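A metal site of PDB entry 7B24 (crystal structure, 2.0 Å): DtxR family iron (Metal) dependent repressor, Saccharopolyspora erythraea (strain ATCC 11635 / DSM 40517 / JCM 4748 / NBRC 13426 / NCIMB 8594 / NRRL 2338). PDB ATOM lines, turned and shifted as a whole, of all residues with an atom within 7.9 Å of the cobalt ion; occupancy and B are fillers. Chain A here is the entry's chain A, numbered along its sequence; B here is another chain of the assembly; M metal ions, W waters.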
ATOM      1  N   ARG A  15       9.713  -9.752  12.710  1.00  0.00           N
ATOM      2  CA  ARG A  15      10.875 -10.437  12.076  1.00  0.00           C
ATOM      3  C   ARG A  15      12.109 -10.326  12.981  1.00  0.00           C
ATOM      4  O   ARG A  15      12.901 -11.272  12.990  1.00  0.00           O
ATOM      5  CB  ARG A  15      11.161  -9.883  10.672  1.00  0.00           C
ATOM      6  CG  ARG A  15      11.661 -10.934   9.695  1.00  0.00           C
ATOM      7  CD  ARG A  15      12.564 -10.353   8.619  1.00  0.00           C
ATOM      8  NE  ARG A  15      13.888 -10.074   9.141  1.00  0.00           N
ATOM      9  CZ  ARG A  15      14.760  -9.213   8.615  1.00  0.00           C
ATOM     10  NH1 ARG A  15      14.450  -8.517   7.534  1.00  0.00           N
ATOM     11  NH2 ARG A  15      15.949  -9.055   9.177  1.00  0.00           N
ATOM     12  N   ASP A  19      14.213 -13.287  14.282  1.00  0.00           N
ATOM     13  CA  ASP A  19      15.691 -13.333  14.092  1.00  0.00           C
ATOM     14  C   ASP A  19      16.371 -13.724  15.405  1.00  0.00           C
ATOM     15  O   ASP A  19      17.256 -14.602  15.376  1.00  0.00           O
ATOM     16  CB  ASP A  19      16.254 -11.990  13.634  1.00  0.00           C
ATOM     17  CG  ASP A  19      15.803 -11.551  12.242  1.00  0.00           C
ATOM     18  OD1 ASP A  19      15.287 -12.408  11.504  1.00  0.00           O
ATOM     19  OD2 ASP A  19      15.965 -10.355  11.936  1.00  0.00           O
ATOM     20  N   MET A  78       9.224 -13.539   6.660  1.00  0.00           N
ATOM     21  CA  MET A  78      10.541 -14.220   6.544  1.00  0.00           C
ATOM     22  C   MET A  78      10.578 -15.056   5.265  1.00  0.00           C
ATOM     23  O   MET A  78      11.653 -15.117   4.632  1.00  0.00           O
ATOM     24  CB  MET A  78      10.813 -15.137   7.752  1.00  0.00           C
ATOM     25  CG  MET A  78      12.240 -15.667   7.789  1.00  0.00           C
ATOM     26  SD  MET A  78      13.490 -14.346   7.773  1.00  0.00           S
ATOM     27  CE  MET A  78      13.583 -13.977   9.528  1.00  0.00           C
ATOM     28  N   HIS A  81      11.050 -12.559   2.479  1.00  0.00           N
ATOM     29  CA  HIS A  81      12.456 -12.085   2.631  1.00  0.00           C
ATOM     30  C   HIS A  81      13.432 -13.044   1.928  1.00  0.00           C
ATOM     31  O   HIS A  81      14.251 -12.547   1.128  1.00  0.00           O
ATOM     32  CB  HIS A  81      12.827 -11.953   4.116  1.00  0.00           C
ATOM     33  CG  HIS A  81      14.205 -11.433   4.328  1.00  0.00           C
ATOM     34  ND1 HIS A  81      14.532 -10.105   4.097  1.00  0.00           N
ATOM     35  CD2 HIS A  81      15.341 -12.051   4.713  1.00  0.00           C
ATOM     36  CE1 HIS A  81      15.818  -9.931   4.359  1.00  0.00           C
ATOM     37  NE2 HIS A  81      16.336 -11.104   4.734  1.00  0.00           N
ATOM     38  N   ARG A  82      13.337 -14.340   2.215  1.00  0.00           N
ATOM     39  CA  ARG A  82      14.339 -15.359   1.808  1.00  0.00           C
ATOM     40  C   ARG A  82      14.100 -15.788   0.348  1.00  0.00           C
ATOM     41  O   ARG A  82      15.080 -16.210  -0.307  1.00  0.00           O
ATOM     42  CB  ARG A  82      14.343 -16.514   2.806  1.00  0.00           C
ATOM     43  CG  ARG A  82      14.876 -16.083   4.168  1.00  0.00           C
ATOM     44  CD  ARG A  82      14.962 -17.154   5.234  1.00  0.00           C
ATOM     45  NE  ARG A  82      15.574 -16.566   6.425  1.00  0.00           N
ATOM     46  CZ  ARG A  82      15.588 -17.092   7.645  1.00  0.00           C
ATOM     47  NH1 ARG A  82      15.037 -18.268   7.879  1.00  0.00           N
ATOM     48  NH2 ARG A  82      16.185 -16.439   8.621  1.00  0.00           N
ATOM     49  N   GLU A  85      15.664 -12.869  -1.608  1.00  0.00           N
ATOM     50  CA  GLU A  85      17.147 -13.042  -1.569  1.00  0.00           C
ATOM     51  C   GLU A  85      17.581 -14.031  -2.662  1.00  0.00           C
ATOM     52  O   GLU A  85      18.558 -13.728  -3.373  1.00  0.00           O
ATOM     53  CB  GLU A  85      17.611 -13.518  -0.191  1.00  0.00           C
ATOM     54  CG  GLU A  85      17.546 -12.434   0.865  1.00  0.00           C
ATOM     55  CD  GLU A  85      18.074 -12.835   2.234  1.00  0.00           C
ATOM     56  OE1 GLU A  85      17.934 -14.018   2.596  1.00  0.00           O
ATOM     57  OE2 GLU A  85      18.621 -11.970   2.932  1.00  0.00           O
ATOM     58  N   VAL A  99      22.353  -7.858  -0.993  1.00  0.00           N
ATOM     59  CA  VAL A  99      21.069  -8.573  -1.253  1.00  0.00           C
ATOM     60  C   VAL A  99      20.123  -8.405  -0.053  1.00  0.00           C
ATOM     61  O   VAL A  99      18.933  -8.106  -0.296  1.00  0.00           O
ATOM     62  CB  VAL A  99      21.316 -10.054  -1.588  1.00  0.00           C
ATOM     63  CG1 VAL A  99      20.092 -10.925  -1.364  1.00  0.00           C
ATOM     64  CG2 VAL A  99      21.841 -10.230  -3.006  1.00  0.00           C
ATOM     65  N   HIS A 100      20.609  -8.596   1.170  1.00  0.00           N
ATOM     66  CA  HIS A 100      19.795  -8.573   2.414  1.00  0.00           C
ATOM     67  C   HIS A 100      19.075  -7.228   2.568  1.00  0.00           C
ATOM     68  O   HIS A 100      17.858  -7.253   2.858  1.00  0.00           O
ATOM     69  CB  HIS A 100      20.638  -8.893   3.657  1.00  0.00           C
ATOM     70  CG  HIS A 100      19.877  -8.705   4.926  1.00  0.00           C
ATOM     71  ND1 HIS A 100      19.000  -9.652   5.413  1.00  0.00           N
ATOM     72  CD2 HIS A 100      19.839  -7.674   5.797  1.00  0.00           C
ATOM     73  CE1 HIS A 100      18.466  -9.220   6.529  1.00  0.00           C
ATOM     74  NE2 HIS A 100      18.961  -8.001   6.791  1.00  0.00           N
ATOM     75  N   LEU A 101      19.793  -6.118   2.399  1.00  0.00           N
ATOM     76  CA  LEU A 101      19.257  -4.736   2.571  1.00  0.00           C
ATOM     77  C   LEU A 101      18.103  -4.523   1.578  1.00  0.00           C
ATOM     78  O   LEU A 101      17.113  -3.872   1.963  1.00  0.00           O
ATOM     79  CB  LEU A 101      20.368  -3.705   2.348  1.00  0.00           C
ATOM     80  CG  LEU A 101      20.023  -2.284   2.797  1.00  0.00           C
ATOM     81  CD1 LEU A 101      20.199  -2.121   4.299  1.00  0.00           C
ATOM     82  CD2 LEU A 101      20.861  -1.254   2.050  1.00  0.00           C
ATOM     83  N   ALA A 103      16.243  -7.089   0.103  1.00  0.00           N
ATOM     84  CA  ALA A 103      15.231  -8.088   0.516  1.00  0.00           C
ATOM     85  C   ALA A 103      14.470  -7.609   1.762  1.00  0.00           C
ATOM     86  O   ALA A 103      13.298  -7.995   1.916  1.00  0.00           O
ATOM     87  CB  ALA A 103      15.911  -9.414   0.760  1.00  0.00           C
ATOM     88  N   CYS A 104      15.102  -6.802   2.612  1.00  0.00           N
ATOM     89  CA  CYS A 104      14.510  -6.260   3.870  1.00  0.00           C
ATOM     90  C   CYS A 104      13.398  -5.253   3.549  1.00  0.00           C
ATOM     91  O   CYS A 104      12.514  -5.067   4.406  1.00  0.00           O
ATOM     92  CB  CYS A 104      15.580  -5.622   4.747  1.00  0.00           C
ATOM     93  SG  CYS A 104      15.085  -5.519   6.491  1.00  0.00           S
ATOM     94  N   GLU A 107      10.373  -7.590   1.262  1.00  0.00           N
ATOM     95  CA  GLU A 107       9.606  -8.544   2.101  1.00  0.00           C
ATOM     96  C   GLU A 107       8.243  -7.952   2.493  1.00  0.00           C
ATOM     97  O   GLU A 107       7.325  -8.748   2.782  1.00  0.00           O
ATOM     98  CB  GLU A 107      10.398  -8.920   3.349  1.00  0.00           C
ATOM     99  CG  GLU A 107      10.657  -7.764   4.298  1.00  0.00           C
ATOM    100  CD  GLU A 107      11.536  -8.094   5.488  1.00  0.00           C
ATOM    101  OE1 GLU A 107      12.063  -9.222   5.547  1.00  0.00           O
ATOM    102  OE2 GLU A 107      11.688  -7.232   6.367  1.00  0.00           O
ATOM    103  N   SER A 128      17.625 -19.826   1.963  1.00  0.00           N
ATOM    104  CA  SER A 128      18.114 -18.536   1.402  1.00  0.00           C
ATOM    105  C   SER A 128      19.553 -18.728   0.922  1.00  0.00           C
ATOM    106  O   SER A 128      20.161 -19.752   1.227  1.00  0.00           O
ATOM    107  CB  SER A 128      18.019 -17.430   2.436  1.00  0.00           C
ATOM    108  OG  SER A 128      19.076 -17.525   3.373  1.00  0.00           O
ATOM    109  N   PRO A 129      20.139 -17.770   0.178  1.00  0.00           N
ATOM    110  CA  PRO A 129      21.533 -17.866  -0.258  1.00  0.00           C
ATOM    111  C   PRO A 129      22.544 -17.944   0.902  1.00  0.00           C
ATOM    112  O   PRO A 129      23.675 -18.283   0.651  1.00  0.00           O
ATOM    113  CB  PRO A 129      21.778 -16.579  -1.059  1.00  0.00           C
ATOM    114  CG  PRO A 129      20.389 -16.108  -1.451  1.00  0.00           C
ATOM    115  CD  PRO A 129      19.501 -16.537  -0.308  1.00  0.00           C
ATOM    116  N   TYR A 130      22.109 -17.625   2.126  1.00  0.00           N
ATOM    117  CA  TYR A 130      22.935 -17.586   3.361  1.00  0.00           C
ATOM    118  C   TYR A 130      22.642 -18.835   4.218  1.00  0.00           C
ATOM    119  O   TYR A 130      23.111 -18.871   5.372  1.00  0.00           O
ATOM    120  CB  TYR A 130      22.694 -16.262   4.071  1.00  0.00           C
ATOM    121  CG  TYR A 130      22.733 -15.093   3.124  1.00  0.00           C
ATOM    122  CD1 TYR A 130      23.932 -14.686   2.555  1.00  0.00           C
ATOM    123  CD2 TYR A 130      21.578 -14.439   2.733  1.00  0.00           C
ATOM    124  CE1 TYR A 130      23.985 -13.638   1.646  1.00  0.00           C
ATOM    125  CE2 TYR A 130      21.618 -13.386   1.828  1.00  0.00           C
ATOM    126  CZ  TYR A 130      22.830 -12.988   1.287  1.00  0.00           C
ATOM    127  OH  TYR A 130      22.872 -11.958   0.391  1.00  0.00           O
ATOM    128  N   ASN A 132      19.849 -20.096   5.455  1.00  0.00           N
ATOM    129  CA  ASN A 132      18.733 -19.999   6.434  1.00  0.00           C
ATOM    130  C   ASN A 132      17.490 -20.652   5.838  1.00  0.00           C
ATOM    131  O   ASN A 132      17.068 -20.272   4.751  1.00  0.00           O
ATOM    132  CB  ASN A 132      18.455 -18.552   6.841  1.00  0.00           C
ATOM    133  CG  ASN A 132      19.695 -17.816   7.292  1.00  0.00           C
ATOM    134  OD1 ASN A 132      20.408 -18.271   8.188  1.00  0.00           O
ATOM    135  ND2 ASN A 132      19.964 -16.666   6.693  1.00  0.00           N
ATOM    136  N   ILE B 172      24.274 -18.299   7.944  1.00  0.00           N
ATOM    137  CA  ILE B 172      24.698 -16.934   8.362  1.00  0.00           C
ATOM    138  C   ILE B 172      23.434 -16.135   8.692  1.00  0.00           C
ATOM    139  O   ILE B 172      22.709 -15.756   7.747  1.00  0.00           O
ATOM    140  CB  ILE B 172      25.543 -16.253   7.260  1.00  0.00           C
ATOM    141  CG1 ILE B 172      26.838 -17.035   6.984  1.00  0.00           C
ATOM    142  CG2 ILE B 172      25.827 -14.801   7.626  1.00  0.00           C
ATOM    143  CD1 ILE B 172      27.585 -16.582   5.756  1.00  0.00           C
ATOM    144  N   ALA B 173      23.181 -15.908   9.987  1.00  0.00           N
ATOM    145  CA  ALA B 173      21.942 -15.276  10.509  1.00  0.00           C
ATOM    146  C   ALA B 173      21.772 -13.871   9.903  1.00  0.00           C
ATOM    147  O   ALA B 173      22.761 -13.294   9.417  1.00  0.00           O
ATOM    148  CB  ALA B 173      21.987 -15.218  12.018  1.00  0.00           C
ATOM    149  N   GLU B 174      20.542 -13.353   9.964  1.00  0.00           N
ATOM    150  CA  GLU B 174      20.123 -12.051   9.361  1.00  0.00           C
ATOM    151  C   GLU B 174      20.918 -10.913  10.025  1.00  0.00           C
ATOM    152  O   GLU B 174      21.170  -9.894   9.348  1.00  0.00           O
ATOM    153  CB  GLU B 174      18.617 -11.835   9.506  1.00  0.00           C
ATOM    154  CG  GLU B 174      17.752 -12.947   8.915  1.00  0.00           C
ATOM    155  CD  GLU B 174      17.811 -13.124   7.406  1.00  0.00           C
ATOM    156  OE1 GLU B 174      17.353 -14.176   6.923  1.00  0.00           O
ATOM    157  OE2 GLU B 174      18.307 -12.212   6.710  1.00  0.00           O
ATOM    158  N   HIS B 175      21.281 -11.079  11.305  1.00  0.00           N
ATOM    159  CA  HIS B 175      22.078 -10.115  12.116  1.00  0.00           C
ATOM    160  C   HIS B 175      23.420  -9.829  11.442  1.00  0.00           C
ATOM    161  O   HIS B 175      23.837  -8.656  11.446  1.00  0.00           O
ATOM    162  CB  HIS B 175      22.243 -10.655  13.541  1.00  0.00           C
ATOM    163  CG  HIS B 175      23.094  -9.807  14.420  1.00  0.00           C
ATOM    164  ND1 HIS B 175      22.820  -8.470  14.660  1.00  0.00           N
ATOM    165  CD2 HIS B 175      24.204 -10.094  15.144  1.00  0.00           C
ATOM    166  CE1 HIS B 175      23.719  -7.969  15.474  1.00  0.00           C
ATOM    167  NE2 HIS B 175      24.582  -8.944  15.786  1.00  0.00           N
ATOM    168  N   GLN B 177      24.151 -10.336   8.170  1.00  0.00           N
ATOM    169  CA  GLN B 177      23.885  -9.846   6.786  1.00  0.00           C
ATOM    170  C   GLN B 177      23.727  -8.313   6.771  1.00  0.00           C
ATOM    171  O   GLN B 177      23.956  -7.718   5.708  1.00  0.00           O
ATOM    172  CB  GLN B 177      22.626 -10.499   6.215  1.00  0.00           C
ATOM    173  CG  GLN B 177      22.756 -12.007   6.019  1.00  0.00           C
ATOM    174  CD  GLN B 177      21.433 -12.638   5.656  1.00  0.00           C
ATOM    175  OE1 GLN B 177      20.677 -12.122   4.834  1.00  0.00           O
ATOM    176  NE2 GLN B 177      21.148 -13.783   6.249  1.00  0.00           N
ATOM    177  N   LEU B 178      23.353  -7.724   7.912  1.00  0.00           N
ATOM    178  CA  LEU B 178      23.092  -6.258   8.064  1.00  0.00           C
ATOM    179  C   LEU B 178      24.402  -5.449   8.023  1.00  0.00           C
ATOM    180  O   LEU B 178      24.307  -4.208   8.012  1.00  0.00           O
ATOM    181  CB  LEU B 178      22.336  -6.007   9.373  1.00  0.00           C
ATOM    182  CG  LEU B 178      20.818  -6.098   9.283  1.00  0.00           C
ATOM    183  CD1 LEU B 178      20.205  -6.342  10.647  1.00  0.00           C
ATOM    184  CD2 LEU B 178      20.246  -4.837   8.642  1.00  0.00           C
ATOM    185  N   MET B 183      30.175  -8.954   5.437  1.00  0.00           N
ATOM    186  CA  MET B 183      29.699  -9.985   4.469  1.00  0.00           C
ATOM    187  C   MET B 183      30.701 -10.122   3.316  1.00  0.00           C
ATOM    188  O   MET B 183      30.938 -11.264   2.887  1.00  0.00           O
ATOM    189  CB  MET B 183      28.311  -9.637   3.921  1.00  0.00           C
ATOM    190  CG  MET B 183      27.187  -9.834   4.925  1.00  0.00           C
ATOM    191  SD  MET B 183      26.983 -11.563   5.445  1.00  0.00           S
ATOM    192  CE  MET B 183      26.227 -12.260   3.984  1.00  0.00           C
HETATM  193 CO    CO M   1      18.511 -11.621   4.903  1.00  0.00          CO
HETATM  194  O   HOH W   1      18.590 -14.970   4.827  1.00  0.00           O
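The cobalt ion is bound by OE2 of Glu 174 of chain B (1.9 Å), OE2 of Glu 85 (2.0 Å), ND1 of His 100 (2.1 Å), OE1 of Gln 177 of chain B (2.2 Å) and NE2 of His 81 (2.2 Å).
Of the 23 residues printed, 5 come within 4 Å of the cobalt ion.
Water W1 lies within hydrogen-bond range of OE1 of Glu 85, OE1 of Glu 174 of chain B, ND2 of Asn 132, OG of Ser 128 and NE2 of Gln 177 of chain B.
OE1 of Glu 174 of chain B lies within salt-bridge range of NE of Arg 82, at 3.0 Å.
The side-chain amide nitrogen (ND2) of Asn 132 sits close to the side-chain amide nitrogen (NE2) of Gln 177 of chain B.
O of Ile 172 of chain B lies within hydrogen-bond range of NE2 of Gln 177 of chain B, at 2.9 Å.
ND1 of His 81 lies within hydrogen-bond range of O of Ala 103, at 3.3 Å.
A ring nitrogen (ND1) of His 81 lies within hydrogen-bond range of the side-chain carboxylate (OE1) of Glu 107 (3.0 Å).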
